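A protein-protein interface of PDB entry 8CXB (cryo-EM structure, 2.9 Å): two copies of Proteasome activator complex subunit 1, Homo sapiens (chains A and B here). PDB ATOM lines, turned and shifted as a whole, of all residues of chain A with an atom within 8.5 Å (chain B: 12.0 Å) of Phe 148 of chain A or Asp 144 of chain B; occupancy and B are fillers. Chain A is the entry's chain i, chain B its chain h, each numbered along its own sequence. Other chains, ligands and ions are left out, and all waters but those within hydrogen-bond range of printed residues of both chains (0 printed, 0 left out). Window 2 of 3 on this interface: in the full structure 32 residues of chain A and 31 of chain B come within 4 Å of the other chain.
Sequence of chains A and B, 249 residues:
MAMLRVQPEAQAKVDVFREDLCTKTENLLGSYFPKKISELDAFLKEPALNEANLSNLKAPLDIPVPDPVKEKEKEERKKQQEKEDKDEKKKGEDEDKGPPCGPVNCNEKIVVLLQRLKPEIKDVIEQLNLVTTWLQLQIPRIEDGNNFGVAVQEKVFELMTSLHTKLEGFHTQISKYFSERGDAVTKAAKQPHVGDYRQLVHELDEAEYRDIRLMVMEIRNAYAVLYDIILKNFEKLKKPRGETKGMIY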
ATOM      1  N   PRO A 140     -13.631   9.376   2.055  1.00  0.00           N
ATOM      2  CA  PRO A 140     -13.716   9.017   3.460  1.00  0.00           C
ATOM      3  C   PRO A 140     -13.614   7.518   3.736  1.00  0.00           C
ATOM      4  O   PRO A 140     -13.470   6.774   2.805  1.00  0.00           O
ATOM      5  CB  PRO A 140     -15.133   9.457   3.776  1.00  0.00           C
ATOM      6  CG  PRO A 140     -15.896   9.103   2.533  1.00  0.00           C
ATOM      7  CD  PRO A 140     -14.944   9.470   1.419  1.00  0.00           C
ATOM      8  N   GLU A 143     -18.018   2.999   3.986  1.00  0.00           N
ATOM      9  CA  GLU A 143     -19.155   2.704   4.888  1.00  0.00           C
ATOM     10  C   GLU A 143     -20.288   2.191   4.012  1.00  0.00           C
ATOM     11  O   GLU A 143     -20.162   2.310   2.796  1.00  0.00           O
ATOM     12  CB  GLU A 143     -19.559   3.940   5.680  1.00  0.00           C
ATOM     13  N   ASP A 144     -21.338   1.635   4.599  1.00  0.00           N
ATOM     14  CA  ASP A 144     -22.401   0.978   3.799  1.00  0.00           C
ATOM     15  C   ASP A 144     -23.491   1.936   3.307  1.00  0.00           C
ATOM     16  O   ASP A 144     -24.384   1.463   2.593  1.00  0.00           O
ATOM     17  CB  ASP A 144     -23.018  -0.130   4.635  1.00  0.00           C
ATOM     18  CG  ASP A 144     -22.732   0.040   6.114  1.00  0.00           C
ATOM     19  OD1 ASP A 144     -21.598  -0.240   6.525  1.00  0.00           O
ATOM     20  OD2 ASP A 144     -23.642   0.459   6.841  1.00  0.00           O
ATOM     21  N   GLY A 145     -23.450   3.214   3.678  1.00  0.00           N
ATOM     22  CA  GLY A 145     -24.535   4.139   3.303  1.00  0.00           C
ATOM     23  C   GLY A 145     -24.070   5.572   3.319  1.00  0.00           C
ATOM     24  O   GLY A 145     -22.967   5.796   3.812  1.00  0.00           O
ATOM     25  N   ASN A 146     -24.885   6.501   2.828  1.00  0.00           N
ATOM     26  CA  ASN A 146     -24.449   7.911   2.687  1.00  0.00           C
ATOM     27  C   ASN A 146     -23.327   7.884   1.658  1.00  0.00           C
ATOM     28  O   ASN A 146     -22.448   8.746   1.716  1.00  0.00           O
ATOM     29  CB  ASN A 146     -24.075   8.574   4.011  1.00  0.00           C
ATOM     30  CG  ASN A 146     -25.108   8.381   5.097  1.00  0.00           C
ATOM     31  OD1 ASN A 146     -26.218   7.936   4.830  1.00  0.00           O
ATOM     32  ND2 ASN A 146     -24.749   8.710   6.325  1.00  0.00           N
ATOM     33  N   ASN A 147     -23.370   6.898   0.769  1.00  0.00           N
ATOM     34  CA  ASN A 147     -22.355   6.761  -0.297  1.00  0.00           C
ATOM     35  C   ASN A 147     -22.532   7.897  -1.295  1.00  0.00           C
ATOM     36  O   ASN A 147     -21.584   8.192  -2.017  1.00  0.00           O
ATOM     37  CB  ASN A 147     -22.387   5.370  -0.914  1.00  0.00           C
ATOM     38  CG  ASN A 147     -21.882   4.315   0.044  1.00  0.00           C
ATOM     39  OD1 ASN A 147     -22.224   3.143  -0.080  1.00  0.00           O
ATOM     40  ND2 ASN A 147     -21.076   4.725   1.008  1.00  0.00           N
ATOM     41  N   PHE A 148     -23.722   8.474  -1.381  1.00  0.00           N
ATOM     42  CA  PHE A 148     -23.813   9.658  -2.261  1.00  0.00           C
ATOM     43  C   PHE A 148     -22.842  10.647  -1.647  1.00  0.00           C
ATOM     44  O   PHE A 148     -22.780  10.749  -0.421  1.00  0.00           O
ATOM     45  CB  PHE A 148     -25.226  10.229  -2.318  1.00  0.00           C
ATOM     46  CG  PHE A 148     -25.365  11.447  -3.191  1.00  0.00           C
ATOM     47  CD1 PHE A 148     -25.533  11.320  -4.559  1.00  0.00           C
ATOM     48  CD2 PHE A 148     -25.313  12.719  -2.649  1.00  0.00           C
ATOM     49  CE1 PHE A 148     -25.651  12.440  -5.365  1.00  0.00           C
ATOM     50  CE2 PHE A 148     -25.425  13.837  -3.458  1.00  0.00           C
ATOM     51  CZ  PHE A 148     -25.596  13.695  -4.813  1.00  0.00           C
ATOM     52  N   GLY A 149     -22.125  11.382  -2.472  1.00  0.00           N
ATOM     53  CA  GLY A 149     -21.064  12.244  -1.944  1.00  0.00           C
ATOM     54  C   GLY A 149     -19.792  11.484  -2.152  1.00  0.00           C
ATOM     55  O   GLY A 149     -18.889  12.026  -2.787  1.00  0.00           O
ATOM     56  N   VAL A 150     -19.746  10.240  -1.697  1.00  0.00           N
ATOM     57  CA  VAL A 150     -18.567   9.416  -2.049  1.00  0.00           C
ATOM     58  C   VAL A 150     -18.713   9.192  -3.545  1.00  0.00           C
ATOM     59  O   VAL A 150     -17.710   9.209  -4.252  1.00  0.00           O
ATOM     60  CB  VAL A 150     -18.530   8.103  -1.261  1.00  0.00           C
ATOM     61  CG1 VAL A 150     -17.242   7.336  -1.504  1.00  0.00           C
ATOM     62  CG2 VAL A 150     -18.729   8.354   0.223  1.00  0.00           C
ATOM     63  N   ALA A 151     -19.945   9.001  -3.995  1.00  0.00           N
ATOM     64  CA  ALA A 151     -20.211   8.811  -5.435  1.00  0.00           C
ATOM     65  C   ALA A 151     -19.875  10.065  -6.231  1.00  0.00           C
ATOM     66  O   ALA A 151     -19.328   9.934  -7.319  1.00  0.00           O
ATOM     67  CB  ALA A 151     -21.655   8.470  -5.608  1.00  0.00           C
ATOM     68  N   VAL A 152     -20.215  11.233  -5.703  1.00  0.00           N
ATOM     69  CA  VAL A 152     -19.889  12.501  -6.402  1.00  0.00           C
ATOM     70  C   VAL A 152     -18.374  12.558  -6.520  1.00  0.00           C
ATOM     71  O   VAL A 152     -17.881  12.878  -7.594  1.00  0.00           O
ATOM     72  CB  VAL A 152     -20.419  13.714  -5.626  1.00  0.00           C
ATOM     73  CG1 VAL A 152     -19.938  15.024  -6.217  1.00  0.00           C
ATOM     74  CG2 VAL A 152     -21.932  13.695  -5.528  1.00  0.00           C
ATOM     75  N   GLN A 153     -17.674  12.176  -5.463  1.00  0.00           N
ATOM     76  CA  GLN A 153     -16.201  12.209  -5.500  1.00  0.00           C
ATOM     77  C   GLN A 153     -15.762  11.255  -6.599  1.00  0.00           C
ATOM     78  O   GLN A 153     -14.877  11.615  -7.366  1.00  0.00           O
ATOM     79  CB  GLN A 153     -15.639  11.814  -4.146  1.00  0.00           C
ATOM     80  CG  GLN A 153     -15.600  12.957  -3.158  1.00  0.00           C
ATOM     81  CD  GLN A 153     -15.037  12.448  -1.860  1.00  0.00           C
ATOM     82  OE1 GLN A 153     -15.353  11.347  -1.426  1.00  0.00           O
ATOM     83  NE2 GLN A 153     -14.187  13.244  -1.241  1.00  0.00           N
ATOM     84  N   GLU A 154     -16.396  10.097  -6.688  1.00  0.00           N
ATOM     85  CA  GLU A 154     -16.009   9.093  -7.706  1.00  0.00           C
ATOM     86  C   GLU A 154     -16.292   9.622  -9.110  1.00  0.00           C
ATOM     87  O   GLU A 154     -15.465   9.401  -9.996  1.00  0.00           O
ATOM     88  CB  GLU A 154     -16.759   7.790  -7.455  1.00  0.00           C
ATOM     89  N   LYS A 155     -17.429  10.272  -9.316  1.00  0.00           N
ATOM     90  CA  LYS A 155     -17.778  10.717 -10.679  1.00  0.00           C
ATOM     91  C   LYS A 155     -16.740  11.728 -11.120  1.00  0.00           C
ATOM     92  O   LYS A 155     -16.308  11.674 -12.267  1.00  0.00           O
ATOM     93  CB  LYS A 155     -19.130  11.422 -10.688  1.00  0.00           C
ATOM     94  CG  LYS A 155     -20.095  10.939 -11.757  1.00  0.00           C
ATOM     95  CD  LYS A 155     -20.674  12.053 -12.597  1.00  0.00           C
ATOM     96  CE  LYS A 155     -19.616  12.851 -13.329  1.00  0.00           C
ATOM     97  NZ  LYS A 155     -18.775  11.987 -14.189  1.00  0.00           N
ATOM     98  N   ASN A 233     -19.401  20.996  -7.429  1.00  0.00           N
ATOM     99  CA  ASN A 233     -19.654  19.928  -6.438  1.00  0.00           C
ATOM    100  C   ASN A 233     -18.680  20.040  -5.271  1.00  0.00           C
ATOM    101  O   ASN A 233     -18.516  19.053  -4.562  1.00  0.00           O
ATOM    102  CB  ASN A 233     -19.549  18.572  -7.115  1.00  0.00           C
ATOM    103  CG  ASN A 233     -20.142  18.570  -8.504  1.00  0.00           C
ATOM    104  OD1 ASN A 233     -21.313  18.877  -8.678  1.00  0.00           O
ATOM    105  ND2 ASN A 233     -19.343  18.221  -9.495  1.00  0.00           N
ATOM    106  N   LYS A 236     -19.769  18.672  -1.652  1.00  0.00           N
ATOM    107  CA  LYS A 236     -19.693  17.204  -1.468  1.00  0.00           C
ATOM    108  C   LYS A 236     -18.241  16.721  -1.514  1.00  0.00           C
ATOM    109  O   LYS A 236     -17.906  15.875  -0.706  1.00  0.00           O
ATOM    110  CB  LYS A 236     -20.652  16.442  -2.375  1.00  0.00           C
ATOM    111  CG  LYS A 236     -22.107  16.490  -1.944  1.00  0.00           C
ATOM    112  CD  LYS A 236     -22.318  15.910  -0.569  1.00  0.00           C
ATOM    113  CE  LYS A 236     -23.776  15.815  -0.181  1.00  0.00           C
ATOM    114  NZ  LYS A 236     -23.950  15.114   1.112  1.00  0.00           N
ATOM    115  N   LYS A 239     -16.626  17.551   1.851  1.00  0.00           N
ATOM    116  CA  LYS A 239     -17.266  16.847   2.990  1.00  0.00           C
ATOM    117  C   LYS A 239     -18.225  15.803   2.449  1.00  0.00           C
ATOM    118  O   LYS A 239     -19.427  16.064   2.438  1.00  0.00           O
ATOM    119  CB  LYS A 239     -18.049  17.829   3.856  1.00  0.00           C
ATOM    120  CG  LYS A 239     -17.199  18.706   4.761  1.00  0.00           C
ATOM    121  CD  LYS A 239     -18.018  19.627   5.630  1.00  0.00           C
ATOM    122  CE  LYS A 239     -17.162  20.602   6.411  1.00  0.00           C
ATOM    123  NZ  LYS A 239     -16.305  21.415   5.514  1.00  0.00           N
ATOM    124  N   PRO A 240     -17.750  14.625   2.022  1.00  0.00           N
ATOM    125  CA  PRO A 240     -18.641  13.683   1.381  1.00  0.00           C
ATOM    126  C   PRO A 240     -19.756  13.184   2.286  1.00  0.00           C
ATOM    127  O   PRO A 240     -20.877  13.170   1.871  1.00  0.00           O
ATOM    128  CB  PRO A 240     -17.743  12.464   1.262  1.00  0.00           C
ATOM    129  CG  PRO A 240     -16.342  13.001   1.241  1.00  0.00           C
ATOM    130  CD  PRO A 240     -16.378  14.169   2.191  1.00  0.00           C
ATOM    131  N   ARG A 241     -19.404  12.773   3.491  1.00  0.00           N
ATOM    132  CA  ARG A 241     -20.400  12.177   4.406  1.00  0.00           C
ATOM    133  C   ARG A 241     -21.384  13.208   4.929  1.00  0.00           C
ATOM    134  O   ARG A 241     -22.554  12.857   5.087  1.00  0.00           O
ATOM    135  CB  ARG A 241     -19.688  11.572   5.611  1.00  0.00           C
ATOM    136  CG  ARG A 241     -18.886  10.319   5.301  1.00  0.00           C
ATOM    137  CD  ARG A 241     -19.760   9.215   4.753  1.00  0.00           C
ATOM    138  NE  ARG A 241     -18.923   8.112   4.316  1.00  0.00           N
ATOM    139  CZ  ARG A 241     -19.358   7.098   3.589  1.00  0.00           C
ATOM    140  NH1 ARG A 241     -20.621   7.059   3.214  1.00  0.00           N
ATOM    141  NH2 ARG A 241     -18.529   6.137   3.229  1.00  0.00           N
ATOM    142  N   GLY A 242     -20.921  14.417   5.218  1.00  0.00           N
ATOM    143  CA  GLY A 242     -21.793  15.404   5.882  1.00  0.00           C
ATOM    144  C   GLY A 242     -21.446  15.398   7.357  1.00  0.00           C
ATOM    145  O   GLY A 242     -20.854  14.403   7.796  1.00  0.00           O
ATOM    146  N   ILE B 139     -23.552  21.026 -17.839  1.00  0.00           N
ATOM    147  CA  ILE B 139     -23.896  19.920 -16.894  1.00  0.00           C
ATOM    148  C   ILE B 139     -23.985  20.496 -15.487  1.00  0.00           C
ATOM    149  O   ILE B 139     -23.038  21.158 -15.066  1.00  0.00           O
ATOM    150  CB  ILE B 139     -22.859  18.789 -16.991  1.00  0.00           C
ATOM    151  CG1 ILE B 139     -22.949  18.061 -18.332  1.00  0.00           C
ATOM    152  CG2 ILE B 139     -22.978  17.821 -15.828  1.00  0.00           C
ATOM    153  CD1 ILE B 139     -22.003  16.895 -18.457  1.00  0.00           C
ATOM    154  N   PRO B 140     -25.048  20.204 -14.718  1.00  0.00           N
ATOM    155  CA  PRO B 140     -25.253  20.823 -13.415  1.00  0.00           C
ATOM    156  C   PRO B 140     -24.545  20.154 -12.238  1.00  0.00           C
ATOM    157  O   PRO B 140     -23.836  19.212 -12.457  1.00  0.00           O
ATOM    158  CB  PRO B 140     -26.763  20.673 -13.270  1.00  0.00           C
ATOM    159  CG  PRO B 140     -27.043  19.328 -13.875  1.00  0.00           C
ATOM    160  CD  PRO B 140     -26.120  19.274 -15.071  1.00  0.00           C
ATOM    161  N   ARG B 141     -24.727  20.694 -11.035  1.00  0.00           N
ATOM    162  CA  ARG B 141     -24.136  20.076  -9.826  1.00  0.00           C
ATOM    163  C   ARG B 141     -24.719  18.677  -9.671  1.00  0.00           C
ATOM    164  O   ARG B 141     -25.934  18.536  -9.822  1.00  0.00           O
ATOM    165  CB  ARG B 141     -24.531  20.894  -8.600  1.00  0.00           C
ATOM    166  CG  ARG B 141     -23.884  20.436  -7.304  1.00  0.00           C
ATOM    167  CD  ARG B 141     -24.566  21.005  -6.077  1.00  0.00           C
ATOM    168  NE  ARG B 141     -25.859  20.381  -5.858  1.00  0.00           N
ATOM    169  CZ  ARG B 141     -27.027  20.939  -6.147  1.00  0.00           C
ATOM    170  NH1 ARG B 141     -27.067  22.157  -6.659  1.00  0.00           N
ATOM    171  NH2 ARG B 141     -28.149  20.285  -5.914  1.00  0.00           N
ATOM    172  N   ILE B 142     -23.889  17.687  -9.364  1.00  0.00           N
ATOM    173  CA  ILE B 142     -24.388  16.288  -9.303  1.00  0.00           C
ATOM    174  C   ILE B 142     -25.362  16.196  -8.139  1.00  0.00           C
ATOM    175  O   ILE B 142     -25.039  16.709  -7.067  1.00  0.00           O
ATOM    176  CB  ILE B 142     -23.217  15.309  -9.165  1.00  0.00           C
ATOM    177  CG1 ILE B 142     -22.083  15.665 -10.127  1.00  0.00           C
ATOM    178  CG2 ILE B 142     -23.687  13.877  -9.355  1.00  0.00           C
ATOM    179  CD1 ILE B 142     -20.847  14.828  -9.945  1.00  0.00           C
ATOM    180  N   GLU B 143     -26.512  15.571  -8.364  1.00  0.00           N
ATOM    181  CA  GLU B 143     -27.550  15.458  -7.312  1.00  0.00           C
ATOM    182  C   GLU B 143     -28.235  14.107  -7.461  1.00  0.00           C
ATOM    183  O   GLU B 143     -28.164  13.539  -8.554  1.00  0.00           O
ATOM    184  CB  GLU B 143     -28.563  16.595  -7.407  1.00  0.00           C
ATOM    185  N   ASP B 144     -28.866  13.620  -6.400  1.00  0.00           N
ATOM    186  CA  ASP B 144     -29.484  12.273  -6.401  1.00  0.00           C
ATOM    187  C   ASP B 144     -30.631  12.148  -7.398  1.00  0.00           C
ATOM    188  O   ASP B 144     -30.757  11.066  -7.980  1.00  0.00           O
ATOM    189  CB  ASP B 144     -30.013  11.951  -5.010  1.00  0.00           C
ATOM    190  CG  ASP B 144     -29.753  13.074  -4.029  1.00  0.00           C
ATOM    191  OD1 ASP B 144     -28.597  13.211  -3.600  1.00  0.00           O
ATOM    192  OD2 ASP B 144     -30.706  13.802  -3.710  1.00  0.00           O
ATOM    193  N   GLY B 145     -31.457  13.179  -7.567  1.00  0.00           N
ATOM    194  CA  GLY B 145     -32.667  13.026  -8.402  1.00  0.00           C
ATOM    195  C   GLY B 145     -32.831  14.104  -9.447  1.00  0.00           C
ATOM    196  O   GLY B 145     -31.967  14.987  -9.494  1.00  0.00           O
ATOM    197  N   ASN B 146     -33.861  13.991 -10.289  1.00  0.00           N
ATOM    198  CA  ASN B 146     -34.070  14.946 -11.404  1.00  0.00           C
ATOM    199  C   ASN B 146     -32.931  14.694 -12.373  1.00  0.00           C
ATOM    200  O   ASN B 146     -32.570  15.599 -13.125  1.00  0.00           O
ATOM    201  CB  ASN B 146     -34.198  16.393 -10.936  1.00  0.00           C
ATOM    202  CG  ASN B 146     -35.593  16.738 -10.469  1.00  0.00           C
ATOM    203  OD1 ASN B 146     -36.576  16.267 -11.035  1.00  0.00           O
ATOM    204  ND2 ASN B 146     -35.689  17.572  -9.449  1.00  0.00           N
ATOM    205  N   ASN B 147     -32.393  13.487 -12.324  1.00  0.00           N
ATOM    206  CA  ASN B 147     -31.259  13.123 -13.197  1.00  0.00           C
ATOM    207  C   ASN B 147     -31.679  13.162 -14.658  1.00  0.00           C
ATOM    208  O   ASN B 147     -30.831  13.483 -15.479  1.00  0.00           O
ATOM    209  CB  ASN B 147     -30.648  11.794 -12.789  1.00  0.00           C
ATOM    210  CG  ASN B 147     -29.793  11.924 -11.547  1.00  0.00           C
ATOM    211  OD1 ASN B 147     -29.466  10.930 -10.905  1.00  0.00           O
ATOM    212  ND2 ASN B 147     -29.432  13.148 -11.203  1.00  0.00           N
ATOM    213  N   PHE B 148     -32.914  12.798 -14.989  1.00  0.00           N
ATOM    214  CA  PHE B 148     -33.241  12.899 -16.427  1.00  0.00           C
ATOM    215  C   PHE B 148     -32.917  14.335 -16.774  1.00  0.00           C
ATOM    216  O   PHE B 148     -33.368  15.234 -16.068  1.00  0.00           O
ATOM    217  CB  PHE B 148     -34.715  12.606 -16.670  1.00  0.00           C
ATOM    218  CG  PHE B 148     -35.058  12.166 -18.067  1.00  0.00           C
ATOM    219  CD1 PHE B 148     -34.794  10.872 -18.484  1.00  0.00           C
ATOM    220  CD2 PHE B 148     -35.658  13.039 -18.958  1.00  0.00           C
ATOM    221  CE1 PHE B 148     -35.110  10.464 -19.769  1.00  0.00           C
ATOM    222  CE2 PHE B 148     -35.973  12.628 -20.242  1.00  0.00           C
ATOM    223  CZ  PHE B 148     -35.696  11.344 -20.644  1.00  0.00           C
ATOM    224  N   GLY B 149     -32.178  14.536 -17.843  1.00  0.00           N
ATOM    225  CA  GLY B 149     -31.707  15.888 -18.144  1.00  0.00           C
ATOM    226  C   GLY B 149     -30.220  15.762 -18.081  1.00  0.00           C
ATOM    227  O   GLY B 149     -29.558  16.071 -19.068  1.00  0.00           O
ATOM    228  N   VAL B 150     -29.714  15.282 -16.957  1.00  0.00           N
ATOM    229  CA  VAL B 150     -28.265  14.974 -16.921  1.00  0.00           C
ATOM    230  C   VAL B 150     -28.109  13.800 -17.874  1.00  0.00           C
ATOM    231  O   VAL B 150     -27.117  13.744 -18.594  1.00  0.00           O
ATOM    232  CB  VAL B 150     -27.783  14.646 -15.505  1.00  0.00           C
ATOM    233  CG1 VAL B 150     -26.271  14.517 -15.444  1.00  0.00           C
ATOM    234  CG2 VAL B 150     -28.263  15.687 -14.511  1.00  0.00           C
ATOM    235  N   ALA B 151     -29.084  12.901 -17.869  1.00  0.00           N
ATOM    236  CA  ALA B 151     -29.047  11.753 -18.791  1.00  0.00           C
ATOM    237  C   ALA B 151     -29.127  12.236 -20.230  1.00  0.00           C
ATOM    238  O   ALA B 151     -28.350  11.758 -21.061  1.00  0.00           O
ATOM    239  CB  ALA B 151     -30.218  10.874 -18.507  1.00  0.00           C
ATOM    240  N   PRO B 240     -30.870  21.509 -17.603  1.00  0.00           N
ATOM    241  CA  PRO B 240     -31.190  20.132 -17.296  1.00  0.00           C
ATOM    242  C   PRO B 240     -32.115  19.934 -16.099  1.00  0.00           C
ATOM    243  O   PRO B 240     -33.034  19.170 -16.197  1.00  0.00           O
ATOM    244  CB  PRO B 240     -29.829  19.637 -16.825  1.00  0.00           C
ATOM    245  CG  PRO B 240     -28.833  20.496 -17.540  1.00  0.00           C
ATOM    246  CD  PRO B 240     -29.462  21.862 -17.475  1.00  0.00           C
ATOM    247  N   ARG B 241     -31.843  20.630 -15.007  1.00  0.00           N
ATOM    248  CA  ARG B 241     -32.634  20.433 -13.770  1.00  0.00           C
ATOM    249  C   ARG B 241     -34.070  20.882 -14.012  1.00  0.00           C
ATOM    250  O   ARG B 241     -34.982  20.233 -13.493  1.00  0.00           O
ATOM    251  CB  ARG B 241     -31.978  21.159 -12.597  1.00  0.00           C
ATOM    252  CG  ARG B 241     -30.652  20.557 -12.167  1.00  0.00           C
ATOM    253  CD  ARG B 241     -30.808  19.090 -11.832  1.00  0.00           C
ATOM    254  NE  ARG B 241     -29.527  18.508 -11.472  1.00  0.00           N
ATOM    255  CZ  ARG B 241     -29.331  17.217 -11.253  1.00  0.00           C
ATOM    256  NH1 ARG B 241     -30.340  16.373 -11.362  1.00  0.00           N
ATOM    257  NH2 ARG B 241     -28.129  16.774 -10.935  1.00  0.00           N
ATOM    258  N   LYS B 245     -38.800  24.535  -8.220  1.00  0.00           N
ATOM    259  CA  LYS B 245     -40.181  24.134  -7.849  1.00  0.00           C
ATOM    260  C   LYS B 245     -40.663  24.896  -6.616  1.00  0.00           C
ATOM    261  O   LYS B 245     -39.935  25.784  -6.153  1.00  0.00           O
ATOM    262  CB  LYS B 245     -40.250  22.617  -7.673  1.00  0.00           C
ATOM    263  CG  LYS B 245     -39.939  21.806  -8.921  1.00  0.00           C
ATOM    264  CD  LYS B 245     -39.778  20.333  -8.636  1.00  0.00           C
ATOM    265  CE  LYS B 245     -39.352  19.543  -9.852  1.00  0.00           C
ATOM    266  NZ  LYS B 245     -38.159  20.142 -10.495  1.00  0.00           N
ATOM    267  N   ILE B 248     -40.805  22.061  -0.819  1.00  0.00           N
ATOM    268  CA  ILE B 248     -41.563  21.312   0.219  1.00  0.00           C
ATOM    269  C   ILE B 248     -41.152  21.846   1.590  1.00  0.00           C
ATOM    270  O   ILE B 248     -42.024  21.975   2.450  1.00  0.00           O
ATOM    271  CB  ILE B 248     -41.295  19.807   0.067  1.00  0.00           C
ATOM    272  CG1 ILE B 248     -39.929  19.551  -0.567  1.00  0.00           C
ATOM    273  CG2 ILE B 248     -42.389  19.143  -0.739  1.00  0.00           C
ATOM    274  CD1 ILE B 248     -39.752  18.144  -1.085  1.00  0.00           C
ATOM    275  N   TYR B 249     -39.868  22.138   1.776  1.00  0.00           N
ATOM    276  CA  TYR B 249     -39.366  22.663   3.066  1.00  0.00           C
ATOM    277  C   TYR B 249     -39.742  24.134   3.157  1.00  0.00           C
ATOM    278  O   TYR B 249     -39.957  24.698   2.075  1.00  0.00           O
ATOM    279  CB  TYR B 249     -37.844  22.565   3.120  1.00  0.00           C
ATOM    280  CG  TYR B 249     -37.259  21.346   2.464  1.00  0.00           C
ATOM    281  CD1 TYR B 249     -37.035  20.189   3.184  1.00  0.00           C
ATOM    282  CD2 TYR B 249     -36.912  21.359   1.126  1.00  0.00           C
ATOM    283  CE1 TYR B 249     -36.492  19.066   2.587  1.00  0.00           C
ATOM    284  CE2 TYR B 249     -36.372  20.245   0.511  1.00  0.00           C
ATOM    285  CZ  TYR B 249     -36.161  19.096   1.246  1.00  0.00           C
ATOM    286  OH  TYR B 249     -35.625  18.000   0.644  1.00  0.00           O
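Among the printed residues, merely in contact across the chains: Phe 148 of chain A with Ile 142 of chain B (3.8 Å), Phe 148 of chain A with Glu 143 of chain B (3.6 Å), Phe 148 of chain A with Asp 144 of chain B (3.2 Å), Val 152 of chain A with Ile 142 of chain B (3.8 Å), Lys 155 of chain A with Ile 142 of chain B (3.8 Å) and Asn 233 of chain A with Arg 141 of chain B (3.3 Å).
The backbone carbonyl oxygen of Asp 144 of chain B sits close to the side-chain amide oxygen of Asn 147 of chain B (3.2 Å). The backbone carbonyl oxygen (O) of Arg 141 of chain B lies within hydrogen-bond range of the guanidinium group (NH2) of Arg 241 of chain B, 3.0 Å away. O of Glu 143 of chain B is in hydrogen-bond range of ND2 of Asn 147 of chain B (3.0 Å).
No residue of chain B comes within 4 Å of Gly 145 of chain A. Asn 146 of chain A touches none of the printed residues of chain B. No residue of chain B comes within 4 Å of Asn 147 of chain A. Of the printed residues of chain B, Phe 148 of chain A touches Ile 142 (3.8 Å), Glu 143 (3.6 Å) and Asp 144 (3.2 Å). Ala 151 of chain A touches none of the printed residues of chain B. Printed residues of chain B within 4 Å of Val 152 of chain A: Ile 142. Printed residues of chain B within 4 Å of Asn 233 of chain A: Arg 141 and Ile 142. No residue of chain B comes within 4 Å of Lys 236 of chain A. No residue of chain B comes within 4 Å of Arg 241 of chain A. Glu 143 of chain B touches one residue of chain A. Of chain A, only Phe 148 (3.2 Å) comes within 4 Å of Asp 144 of chain B. Gly 145 of chain B touches none of the printed residues of chain A. The nearest residue of chain B that does not touch Phe 148 of chain A is Gly 145 of chain B (6.3 Å). The nearest residue of chain A that does not touch Asp 144 of chain B is Lys 236 of chain A (6.5 Å).
Phe 148 of chain A touches Glu 143 of chain B, but with the chains exchanged Glu 143 of chain A does not touch Phe 148 of chain B (24.3 Å). Phe 148 of chain A touches Asp 144 of chain B, but with the chains exchanged Asp 144 of chain A does not touch Phe 148 of chain B (22.6 Å). Positions printed for both chains: 140, 143, 144, 145, 146, 147, 148, 149, 150, 151, 240 and 241. Of the 7 pairs that touch across the chains among the printed residues, none has its exchanged pair printed and touching as well.
Hydrophobic or aromatic side chains of chain A within 4 Å of the printed part of chain B: Phe 148 and Val 152. Along chain A the printed residues that touch a printed residue of chain B span positions 148 to 233. Of the 18 printed residues of chain B, 4 touch a printed residue of chain A. Hydrophobic or aromatic side chains of chain B within 4 Å of the printed part of chain A: Ile 142. Among the printed residues, no Asp or Glu carboxylate lies within 4 Å of a Lys or Arg side-chain nitrogen of the other chain.
The side-chain amide oxygen (OD1) of Asn 233 of chain A lies within hydrogen-bond range of the backbone NH (N) of Ile 142 of chain B, at 2.9 Å.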
